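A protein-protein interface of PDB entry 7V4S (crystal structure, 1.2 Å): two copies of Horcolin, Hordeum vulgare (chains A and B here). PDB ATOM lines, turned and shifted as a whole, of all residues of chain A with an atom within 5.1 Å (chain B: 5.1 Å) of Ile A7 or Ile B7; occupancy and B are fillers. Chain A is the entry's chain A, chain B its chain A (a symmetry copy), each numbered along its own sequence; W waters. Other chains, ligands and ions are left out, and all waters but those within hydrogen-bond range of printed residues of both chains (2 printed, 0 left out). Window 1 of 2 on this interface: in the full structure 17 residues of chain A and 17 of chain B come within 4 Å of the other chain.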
ATOM      1  N   VAL A   5      -1.717 -19.660  -5.747  1.00  0.00           N
ATOM      2  CA  VAL A   5      -1.319 -18.358  -5.156  1.00  0.00           C
ATOM      3  C   VAL A   5       0.168 -18.481  -4.824  1.00  0.00           C
ATOM      4  O   VAL A   5       0.596 -19.568  -4.364  1.00  0.00           O
ATOM      5  CB  VAL A   5      -2.193 -18.099  -3.923  1.00  0.00           C
ATOM      6  CG1 VAL A   5      -1.591 -17.063  -2.971  1.00  0.00           C
ATOM      7  CG2 VAL A   5      -3.623 -17.806  -4.337  1.00  0.00           C
ATOM      8  N   LYS A   6       0.922 -17.405  -4.930  1.00  0.00           N
ATOM      9  CA  LYS A   6       2.349 -17.353  -4.598  1.00  0.00           C
ATOM     10  C   LYS A   6       2.538 -16.275  -3.547  1.00  0.00           C
ATOM     11  O   LYS A   6       2.176 -15.113  -3.817  1.00  0.00           O
ATOM     12  CB  LYS A   6       3.158 -17.061  -5.843  1.00  0.00           C
ATOM     13  CG  LYS A   6       4.647 -17.099  -5.619  1.00  0.00           C
ATOM     14  CD  LYS A   6       5.488 -16.807  -6.850  1.00  0.00           C
ATOM     15  CE  LYS A   6       6.954 -17.018  -6.595  1.00  0.00           C
ATOM     16  NZ  LYS A   6       7.794 -16.594  -7.741  1.00  0.00           N
ATOM     17  N   ILE A   7       3.027 -16.630  -2.368  1.00  0.00           N
ATOM     18  CA  ILE A   7       3.171 -15.653  -1.278  1.00  0.00           C
ATOM     19  C   ILE A   7       4.547 -15.808  -0.660  1.00  0.00           C
ATOM     20  O   ILE A   7       5.036 -16.965  -0.522  1.00  0.00           O
ATOM     21  CB  ILE A   7       2.103 -15.744  -0.182  1.00  0.00           C
ATOM     22  CG1 ILE A   7       2.025 -17.116   0.480  1.00  0.00           C
ATOM     23  CG2 ILE A   7       0.721 -15.346  -0.706  1.00  0.00           C
ATOM     24  CD1 ILE A   7       1.143 -17.143   1.759  1.00  0.00           C
ATOM     25  N   GLY A   8       5.073 -14.704  -0.196  1.00  0.00           N
ATOM     26  CA  GLY A   8       6.352 -14.705   0.512  1.00  0.00           C
ATOM     27  C   GLY A   8       7.412 -13.962  -0.251  1.00  0.00           C
ATOM     28  O   GLY A   8       7.090 -13.120  -1.100  1.00  0.00           O
ATOM     29  N   PRO A   9       8.705 -14.220   0.027  1.00  0.00           N
ATOM     30  CA  PRO A   9       9.180 -15.224   0.979  1.00  0.00           C
ATOM     31  C   PRO A   9       9.413 -14.571   2.337  1.00  0.00           C
ATOM     32  O   PRO A   9       9.275 -13.371   2.545  1.00  0.00           O
ATOM     33  CB  PRO A   9      10.488 -15.650   0.274  1.00  0.00           C
ATOM     34  CG  PRO A   9      11.025 -14.398  -0.328  1.00  0.00           C
ATOM     35  CD  PRO A   9       9.813 -13.555  -0.670  1.00  0.00           C
ATOM     36  N   TRP A  10       9.785 -15.450   3.248  1.00  0.00           N
ATOM     37  CA  TRP A  10      10.189 -15.110   4.641  1.00  0.00           C
ATOM     38  C   TRP A  10      11.667 -15.477   4.792  1.00  0.00           C
ATOM     39  O   TRP A  10      11.999 -16.666   4.550  1.00  0.00           O
ATOM     40  CB  TRP A  10       9.316 -15.843   5.670  1.00  0.00           C
ATOM     41  CG  TRP A  10       7.904 -15.364   5.606  1.00  0.00           C
ATOM     42  CD1 TRP A  10       7.394 -14.270   6.245  1.00  0.00           C
ATOM     43  CD2 TRP A  10       6.860 -15.826   4.740  1.00  0.00           C
ATOM     44  NE1 TRP A  10       6.071 -14.082   5.885  1.00  0.00           N
ATOM     45  CE2 TRP A  10       5.737 -14.993   4.927  1.00  0.00           C
ATOM     46  CE3 TRP A  10       6.752 -16.853   3.823  1.00  0.00           C
ATOM     47  CZ2 TRP A  10       4.511 -15.180   4.305  1.00  0.00           C
ATOM     48  CZ3 TRP A  10       5.550 -17.015   3.169  1.00  0.00           C
ATOM     49  CH2 TRP A  10       4.463 -16.189   3.390  1.00  0.00           C
ATOM     50  N   VAL A 118       2.089 -19.668   8.458  1.00  0.00           N
ATOM     51  CA  VAL A 118       1.041 -19.646   7.406  1.00  0.00           C
ATOM     52  C   VAL A 118       0.115 -20.844   7.596  1.00  0.00           C
ATOM     53  O   VAL A 118       0.397 -21.954   7.105  1.00  0.00           O
ATOM     54  CB  VAL A 118       1.626 -19.601   5.987  1.00  0.00           C
ATOM     55  CG1 VAL A 118       0.502 -19.617   4.977  1.00  0.00           C
ATOM     56  CG2 VAL A 118       2.494 -18.347   5.808  1.00  0.00           C
ATOM     57  N   PRO A 119      -0.971 -20.693   8.379  1.00  0.00           N
ATOM     58  CA  PRO A 119      -1.997 -21.729   8.503  1.00  0.00           C
ATOM     59  C   PRO A 119      -2.940 -21.619   7.297  1.00  0.00           C
ATOM     60  O   PRO A 119      -3.423 -20.549   6.975  1.00  0.00           O
ATOM     61  CB  PRO A 119      -2.724 -21.400   9.806  1.00  0.00           C
ATOM     62  CG  PRO A 119      -2.096 -20.096  10.292  1.00  0.00           C
ATOM     63  CD  PRO A 119      -1.280 -19.517   9.169  1.00  0.00           C
ATOM     64  N   VAL A 120      -3.075 -22.732   6.599  1.00  0.00           N
ATOM     65  CA  VAL A 120      -3.983 -22.787   5.418  1.00  0.00           C
ATOM     66  C   VAL A 120      -5.277 -23.471   5.854  1.00  0.00           C
ATOM     67  O   VAL A 120      -5.208 -24.580   6.300  1.00  0.00           O
ATOM     68  CB  VAL A 120      -3.347 -23.439   4.171  1.00  0.00           C
ATOM     69  CG1 VAL A 120      -4.258 -23.254   2.966  1.00  0.00           C
ATOM     70  CG2 VAL A 120      -1.953 -22.892   3.853  1.00  0.00           C
ATOM     71  N   LEU A 121      -6.397 -22.794   5.609  1.00  0.00           N
ATOM     72  CA  LEU A 121      -7.657 -23.331   6.144  1.00  0.00           C
ATOM     73  C   LEU A 121      -8.538 -23.857   5.006  1.00  0.00           C
ATOM     74  O   LEU A 121      -8.230 -23.711   3.834  1.00  0.00           O
ATOM     75  CB  LEU A 121      -8.361 -22.191   6.880  1.00  0.00           C
ATOM     76  CG  LEU A 121      -7.542 -21.519   7.984  1.00  0.00           C
ATOM     77  CD1 LEU A 121      -8.285 -20.293   8.560  1.00  0.00           C
ATOM     78  CD2 LEU A 121      -7.110 -22.510   9.061  1.00  0.00           C
ATOM     79  N   PHE A 130       9.310 -21.605  -3.217  1.00  0.00           N
ATOM     80  CA  PHE A 130      10.320 -20.759  -3.899  1.00  0.00           C
ATOM     81  C   PHE A 130      11.150 -20.129  -2.751  1.00  0.00           C
ATOM     82  O   PHE A 130      10.840 -20.336  -1.579  1.00  0.00           O
ATOM     83  CB  PHE A 130       9.692 -19.712  -4.818  1.00  0.00           C
ATOM     84  CG  PHE A 130       8.925 -18.642  -4.077  1.00  0.00           C
ATOM     85  CD1 PHE A 130       7.621 -18.896  -3.669  1.00  0.00           C
ATOM     86  CD2 PHE A 130       9.461 -17.387  -3.848  1.00  0.00           C
ATOM     87  CE1 PHE A 130       6.899 -17.911  -3.020  1.00  0.00           C
ATOM     88  CE2 PHE A 130       8.745 -16.397  -3.189  1.00  0.00           C
ATOM     89  CZ  PHE A 130       7.439 -16.664  -2.823  1.00  0.00           C
ATOM     90  N   GLY A 141       9.328 -19.261   0.504  1.00  0.00           N
ATOM     91  CA  GLY A 141       8.006 -18.760   0.127  1.00  0.00           C
ATOM     92  C   GLY A 141       7.168 -19.950  -0.317  1.00  0.00           C
ATOM     93  O   GLY A 141       7.712 -21.037  -0.564  1.00  0.00           O
ATOM     94  N   PHE A 142       5.864 -19.761  -0.453  1.00  0.00           N
ATOM     95  CA  PHE A 142       4.944 -20.895  -0.715  1.00  0.00           C
ATOM     96  C   PHE A 142       4.019 -20.643  -1.901  1.00  0.00           C
ATOM     97  O   PHE A 142       3.596 -19.534  -2.179  1.00  0.00           O
ATOM     98  CB  PHE A 142       4.002 -21.112   0.484  1.00  0.00           C
ATOM     99  CG  PHE A 142       4.739 -21.202   1.788  1.00  0.00           C
ATOM    100  CD1 PHE A 142       5.771 -22.112   1.968  1.00  0.00           C
ATOM    101  CD2 PHE A 142       4.452 -20.327   2.813  1.00  0.00           C
ATOM    102  CE1 PHE A 142       6.503 -22.124   3.145  1.00  0.00           C
ATOM    103  CE2 PHE A 142       5.176 -20.359   3.990  1.00  0.00           C
ATOM    104  CZ  PHE A 142       6.185 -21.277   4.176  1.00  0.00           C
ATOM    105  N   ILE A 144       0.341 -21.997  -2.918  1.00  0.00           N
ATOM    106  CA  ILE A 144      -0.846 -22.501  -2.170  1.00  0.00           C
ATOM    107  C   ILE A 144      -2.050 -22.664  -3.112  1.00  0.00           C
ATOM    108  O   ILE A 144      -2.296 -21.836  -3.913  1.00  0.00           O
ATOM    109  CB  ILE A 144      -1.177 -21.558  -0.987  1.00  0.00           C
ATOM    110  CG1 ILE A 144       0.063 -21.295  -0.121  1.00  0.00           C
ATOM    111  CG2 ILE A 144      -2.340 -22.114  -0.188  1.00  0.00           C
ATOM    112  CD1 ILE A 144      -0.145 -20.386   1.033  1.00  0.00           C
ATOM    113  N   VAL B   5      -8.063 -18.864  -1.585  1.00  0.00           N
ATOM    114  CA  VAL B   5      -7.271 -19.482  -0.493  1.00  0.00           C
ATOM    115  C   VAL B   5      -7.626 -18.708   0.778  1.00  0.00           C
ATOM    116  O   VAL B   5      -7.780 -17.464   0.703  1.00  0.00           O
ATOM    117  CB  VAL B   5      -5.785 -19.389  -0.859  1.00  0.00           C
ATOM    118  CG1 VAL B   5      -4.859 -19.548   0.349  1.00  0.00           C
ATOM    119  CG2 VAL B   5      -5.464 -20.319  -2.014  1.00  0.00           C
ATOM    120  N   LYS B   6      -7.646 -19.363   1.921  1.00  0.00           N
ATOM    121  CA  LYS B   6      -7.916 -18.751   3.226  1.00  0.00           C
ATOM    122  C   LYS B   6      -6.728 -19.037   4.124  1.00  0.00           C
ATOM    123  O   LYS B   6      -6.411 -20.226   4.329  1.00  0.00           O
ATOM    124  CB  LYS B   6      -9.196 -19.312   3.805  1.00  0.00           C
ATOM    125  CG  LYS B   6      -9.614 -18.659   5.096  1.00  0.00           C
ATOM    126  CD  LYS B   6     -10.895 -19.205   5.705  1.00  0.00           C
ATOM    127  CE  LYS B   6     -11.337 -18.405   6.898  1.00  0.00           C
ATOM    128  NZ  LYS B   6     -12.500 -19.015   7.587  1.00  0.00           N
ATOM    129  N   ILE B   7      -6.043 -18.009   4.604  1.00  0.00           N
ATOM    130  CA  ILE B   7      -4.838 -18.210   5.422  1.00  0.00           C
ATOM    131  C   ILE B   7      -4.917 -17.310   6.640  1.00  0.00           C
ATOM    132  O   ILE B   7      -5.395 -16.147   6.518  1.00  0.00           O
ATOM    133  CB  ILE B   7      -3.512 -17.971   4.691  1.00  0.00           C
ATOM    134  CG1 ILE B   7      -3.392 -16.575   4.090  1.00  0.00           C
ATOM    135  CG2 ILE B   7      -3.268 -19.022   3.606  1.00  0.00           C
ATOM    136  CD1 ILE B   7      -1.962 -16.233   3.584  1.00  0.00           C
ATOM    137  N   GLY B   8      -4.353 -17.788   7.718  1.00  0.00           N
ATOM    138  CA  GLY B   8      -4.262 -17.000   8.947  1.00  0.00           C
ATOM    139  C   GLY B   8      -5.078 -17.603  10.056  1.00  0.00           C
ATOM    140  O   GLY B   8      -5.380 -18.804  10.023  1.00  0.00           O
ATOM    141  N   PRO B   9      -5.447 -16.814  11.085  1.00  0.00           N
ATOM    142  CA  PRO B   9      -5.175 -15.382  11.190  1.00  0.00           C
ATOM    143  C   PRO B   9      -3.889 -15.162  11.981  1.00  0.00           C
ATOM    144  O   PRO B   9      -3.244 -16.070  12.490  1.00  0.00           O
ATOM    145  CB  PRO B   9      -6.443 -14.933  11.951  1.00  0.00           C
ATOM    146  CG  PRO B   9      -6.737 -16.045  12.897  1.00  0.00           C
ATOM    147  CD  PRO B   9      -6.253 -17.305  12.210  1.00  0.00           C
ATOM    148  N   TRP B  10      -3.567 -13.884  12.051  1.00  0.00           N
ATOM    149  CA  TRP B  10      -2.428 -13.338  12.841  1.00  0.00           C
ATOM    150  C   TRP B  10      -3.018 -12.460  13.948  1.00  0.00           C
ATOM    151  O   TRP B  10      -3.765 -11.510  13.600  1.00  0.00           O
ATOM    152  CB  TRP B  10      -1.459 -12.550  11.949  1.00  0.00           C
ATOM    153  CG  TRP B  10      -0.783 -13.452  10.971  1.00  0.00           C
ATOM    154  CD1 TRP B  10       0.341 -14.193  11.200  1.00  0.00           C
ATOM    155  CD2 TRP B  10      -1.261 -13.864   9.685  1.00  0.00           C
ATOM    156  NE1 TRP B  10       0.628 -14.976  10.095  1.00  0.00           N
ATOM    157  CE2 TRP B  10      -0.366 -14.828   9.174  1.00  0.00           C
ATOM    158  CE3 TRP B  10      -2.350 -13.525   8.906  1.00  0.00           C
ATOM    159  CZ2 TRP B  10      -0.469 -15.405   7.916  1.00  0.00           C
ATOM    160  CZ3 TRP B  10      -2.482 -14.129   7.675  1.00  0.00           C
ATOM    161  CH2 TRP B  10      -1.575 -15.058   7.199  1.00  0.00           C
ATOM    162  N   VAL B 118       2.478 -10.614   4.507  1.00  0.00           N
ATOM    163  CA  VAL B 118       2.011 -11.507   3.415  1.00  0.00           C
ATOM    164  C   VAL B 118       2.130 -10.772   2.082  1.00  0.00           C
ATOM    165  O   VAL B 118       1.217 -10.025   1.681  1.00  0.00           O
ATOM    166  CB  VAL B 118       0.588 -12.033   3.648  1.00  0.00           C
ATOM    167  CG1 VAL B 118       0.173 -12.900   2.483  1.00  0.00           C
ATOM    168  CG2 VAL B 118       0.521 -12.827   4.961  1.00  0.00           C
ATOM    169  N   PRO B 119       3.281 -10.886   1.391  1.00  0.00           N
ATOM    170  CA  PRO B 119       3.438 -10.349   0.040  1.00  0.00           C
ATOM    171  C   PRO B 119       2.829 -11.350  -0.951  1.00  0.00           C
ATOM    172  O   PRO B 119       3.117 -12.532  -0.904  1.00  0.00           O
ATOM    173  CB  PRO B 119       4.949 -10.228  -0.155  1.00  0.00           C
ATOM    174  CG  PRO B 119       5.561 -10.819   1.113  1.00  0.00           C
ATOM    175  CD  PRO B 119       4.481 -11.550   1.863  1.00  0.00           C
ATOM    176  N   VAL B 120       1.906 -10.845  -1.749  1.00  0.00           N
ATOM    177  CA  VAL B 120       1.247 -11.690  -2.784  1.00  0.00           C
ATOM    178  C   VAL B 120       1.899 -11.375  -4.130  1.00  0.00           C
ATOM    179  O   VAL B 120       1.867 -10.244  -4.522  1.00  0.00           O
ATOM    180  CB  VAL B 120      -0.291 -11.556  -2.814  1.00  0.00           C
ATOM    181  CG1 VAL B 120      -0.887 -12.607  -3.740  1.00  0.00           C
ATOM    182  CG2 VAL B 120      -0.929 -11.669  -1.427  1.00  0.00           C
ATOM    183  N   LEU B 121       2.372 -12.424  -4.800  1.00  0.00           N
ATOM    184  CA  LEU B 121       3.144 -12.167  -6.025  1.00  0.00           C
ATOM    185  C   LEU B 121       2.348 -12.604  -7.259  1.00  0.00           C
ATOM    186  O   LEU B 121       1.281 -13.187  -7.162  1.00  0.00           O
ATOM    187  CB  LEU B 121       4.444 -12.964  -5.918  1.00  0.00           C
ATOM    188  CG  LEU B 121       5.286 -12.682  -4.672  1.00  0.00           C
ATOM    189  CD1 LEU B 121       6.495 -13.641  -4.589  1.00  0.00           C
ATOM    190  CD2 LEU B 121       5.686 -11.214  -4.571  1.00  0.00           C
ATOM    191  N   PHE B 130     -10.992 -12.266   7.342  1.00  0.00           N
ATOM    192  CA  PHE B 130     -11.682 -12.929   8.475  1.00  0.00           C
ATOM    193  C   PHE B 130     -10.822 -12.588   9.718  1.00  0.00           C
ATOM    194  O   PHE B 130      -9.773 -11.957   9.591  1.00  0.00           O
ATOM    195  CB  PHE B 130     -11.850 -14.433   8.267  1.00  0.00           C
ATOM    196  CG  PHE B 130     -10.547 -15.195   8.287  1.00  0.00           C
ATOM    197  CD1 PHE B 130      -9.766 -15.242   7.138  1.00  0.00           C
ATOM    198  CD2 PHE B 130     -10.133 -15.905   9.401  1.00  0.00           C
ATOM    199  CE1 PHE B 130      -8.587 -15.964   7.136  1.00  0.00           C
ATOM    200  CE2 PHE B 130      -8.946 -16.625   9.408  1.00  0.00           C
ATOM    201  CZ  PHE B 130      -8.206 -16.682   8.243  1.00  0.00           C
ATOM    202  N   GLY B 141      -7.029 -12.325   9.251  1.00  0.00           N
ATOM    203  CA  GLY B 141      -6.649 -13.366   8.296  1.00  0.00           C
ATOM    204  C   GLY B 141      -7.102 -12.917   6.914  1.00  0.00           C
ATOM    205  O   GLY B 141      -7.904 -11.979   6.796  1.00  0.00           O
ATOM    206  N   PHE B 142      -6.630 -13.585   5.872  1.00  0.00           N
ATOM    207  CA  PHE B 142      -6.876 -13.121   4.484  1.00  0.00           C
ATOM    208  C   PHE B 142      -7.427 -14.220   3.582  1.00  0.00           C
ATOM    209  O   PHE B 142      -7.112 -15.391   3.708  1.00  0.00           O
ATOM    210  CB  PHE B 142      -5.557 -12.686   3.820  1.00  0.00           C
ATOM    211  CG  PHE B 142      -4.775 -11.724   4.664  1.00  0.00           C
ATOM    212  CD1 PHE B 142      -5.348 -10.551   5.133  1.00  0.00           C
ATOM    213  CD2 PHE B 142      -3.488 -12.025   5.055  1.00  0.00           C
ATOM    214  CE1 PHE B 142      -4.645  -9.715   5.987  1.00  0.00           C
ATOM    215  CE2 PHE B 142      -2.788 -11.175   5.891  1.00  0.00           C
ATOM    216  CZ  PHE B 142      -3.350 -10.000   6.337  1.00  0.00           C
ATOM    217  N   ILE B 144      -7.288 -14.899  -0.407  1.00  0.00           N
ATOM    218  CA  ILE B 144      -6.352 -14.540  -1.510  1.00  0.00           C
ATOM    219  C   ILE B 144      -6.728 -15.283  -2.802  1.00  0.00           C
ATOM    220  O   ILE B 144      -7.025 -16.423  -2.769  1.00  0.00           O
ATOM    221  CB  ILE B 144      -4.890 -14.833  -1.093  1.00  0.00           C
ATOM    222  CG1 ILE B 144      -4.560 -14.194   0.263  1.00  0.00           C
ATOM    223  CG2 ILE B 144      -3.939 -14.398  -2.191  1.00  0.00           C
ATOM    224  CD1 ILE B 144      -3.183 -14.431   0.763  1.00  0.00           C
HETATM  225  O   HOH W   1      -0.344 -15.167  -6.186  1.00  0.00           O
HETATM  226  O   HOH W   2      -7.435 -22.206   1.685  1.00  0.00           O
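The backbone NH (N) of Gly A8 sits at hydrogen-bond distance from the backbone carbonyl oxygen (O) of Pro B119.
The backbone carbonyl oxygen (O) of Lys A6 lies within hydrogen-bond range of the backbone NH (N) of Leu B121 (2.9 Å).
N of Leu A121 sits at hydrogen-bond distance from O of Lys B6.
O of Pro A119 lies within hydrogen-bond range of N of Gly B8 (3.0 Å).
O of Val B5 sits at hydrogen-bond distance from N of Ile B144 (2.8 Å).
The backbone carbonyl oxygen (O) of Ile B7 lies within hydrogen-bond range of the backbone NH (N) of Phe B142.
The backbone NH (N) of Ile A144 is in hydrogen-bond range of the backbone carbonyl oxygen (O) of Val A5 (2.8 Å).
The backbone carbonyl oxygen (O) of Ile A7 sits at hydrogen-bond distance from the backbone NH (N) of Phe A142, 2.9 Å away.
O of Phe B130 is in hydrogen-bond range of N of Gly B141 (2.8 Å).
The backbone carbonyl oxygen (O) of Phe A130 sits at hydrogen-bond distance from the backbone NH (N) of Gly A141, at 2.8 Å.
Ile B144 touches Val A5.
Val B120 touches Lys A6 (CA to O, 3.7 Å).
CD1 of Ile A7 touches CD1 of Ile B7, 3.7 Å away.
Ile A7 touches Pro B119.
Gly A8 touches Leu B121 (O to CD1, 3.6 Å).
Pro A119 touches Ile B7.
CA of Val A120 touches O of Lys B6 (3.7 Å).
O of Gly B8 touches CD1 of Leu A121, at 3.6 Å.
CZ of Phe B130 touches CD1 of Leu A121, at 3.6 Å.
Ile A144 touches Val B5.
Printed residues of chain B within 4 Å of Ile A7: Ile B7 and Pro B119.
Of chain A, only Ile A7 (3.7 Å) and Pro A119 (3.1 Å) come within 4 Å of Ile B7.
Of the printed residues of chain B, Pro A119 touches Ile B7 and Gly B8.
Of the printed residues of chain A, Val B120 touches Lys A6 (3.7 Å).
Of the printed residues of chain B, Ile A144 touches Val B5.
Of the printed residues of chain A, Leu B121 touches Lys A6, Gly A8 and Phe A130.
Printed residues of chain B within 4 Å of Leu A121: Lys B6 (2.9 Å), Gly B8 (3.6 Å) and Phe B130 (3.6 Å).
The nearest residue of chain A that does not touch Ile B7 is Val A118 (4.1 Å).
Of the 14 printed residues of chain A, 9 touch a printed residue of chain B.
Hydrophobic or aromatic side chains of chain A that line the printed part of chain B: Val A5, Ile A7, Pro A119, Val A120, Leu A121, Phe A130 and Ile A144.
Along chain B the printed residues that touch a printed residue of chain A span positions 5 to 144.
Val A5 touches Ile B144, and with the chains exchanged Ile A144 touches Val B5.
Lys A6 touches Val B120, and with the chains exchanged Val A120 touches Lys B6.
Ile A7 touches Pro B119, and with the chains exchanged Pro A119 touches Ile B7.
Gly A8 touches Pro B119, and with the chains exchanged Pro A119 touches Gly B8.
14 positions are printed for both chains.
Of the 16 pairs that touch across the chains among the printed residues, 16 have their exchanged pair printed and touching as well.
Water W1 bridges the backbone carbonyl oxygen (O) of Leu B121 and the backbone NH (N) of Lys A6.
Water W2 bridges O of Leu A121 (2.7 Å) and N of Lys B6 (2.9 Å).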
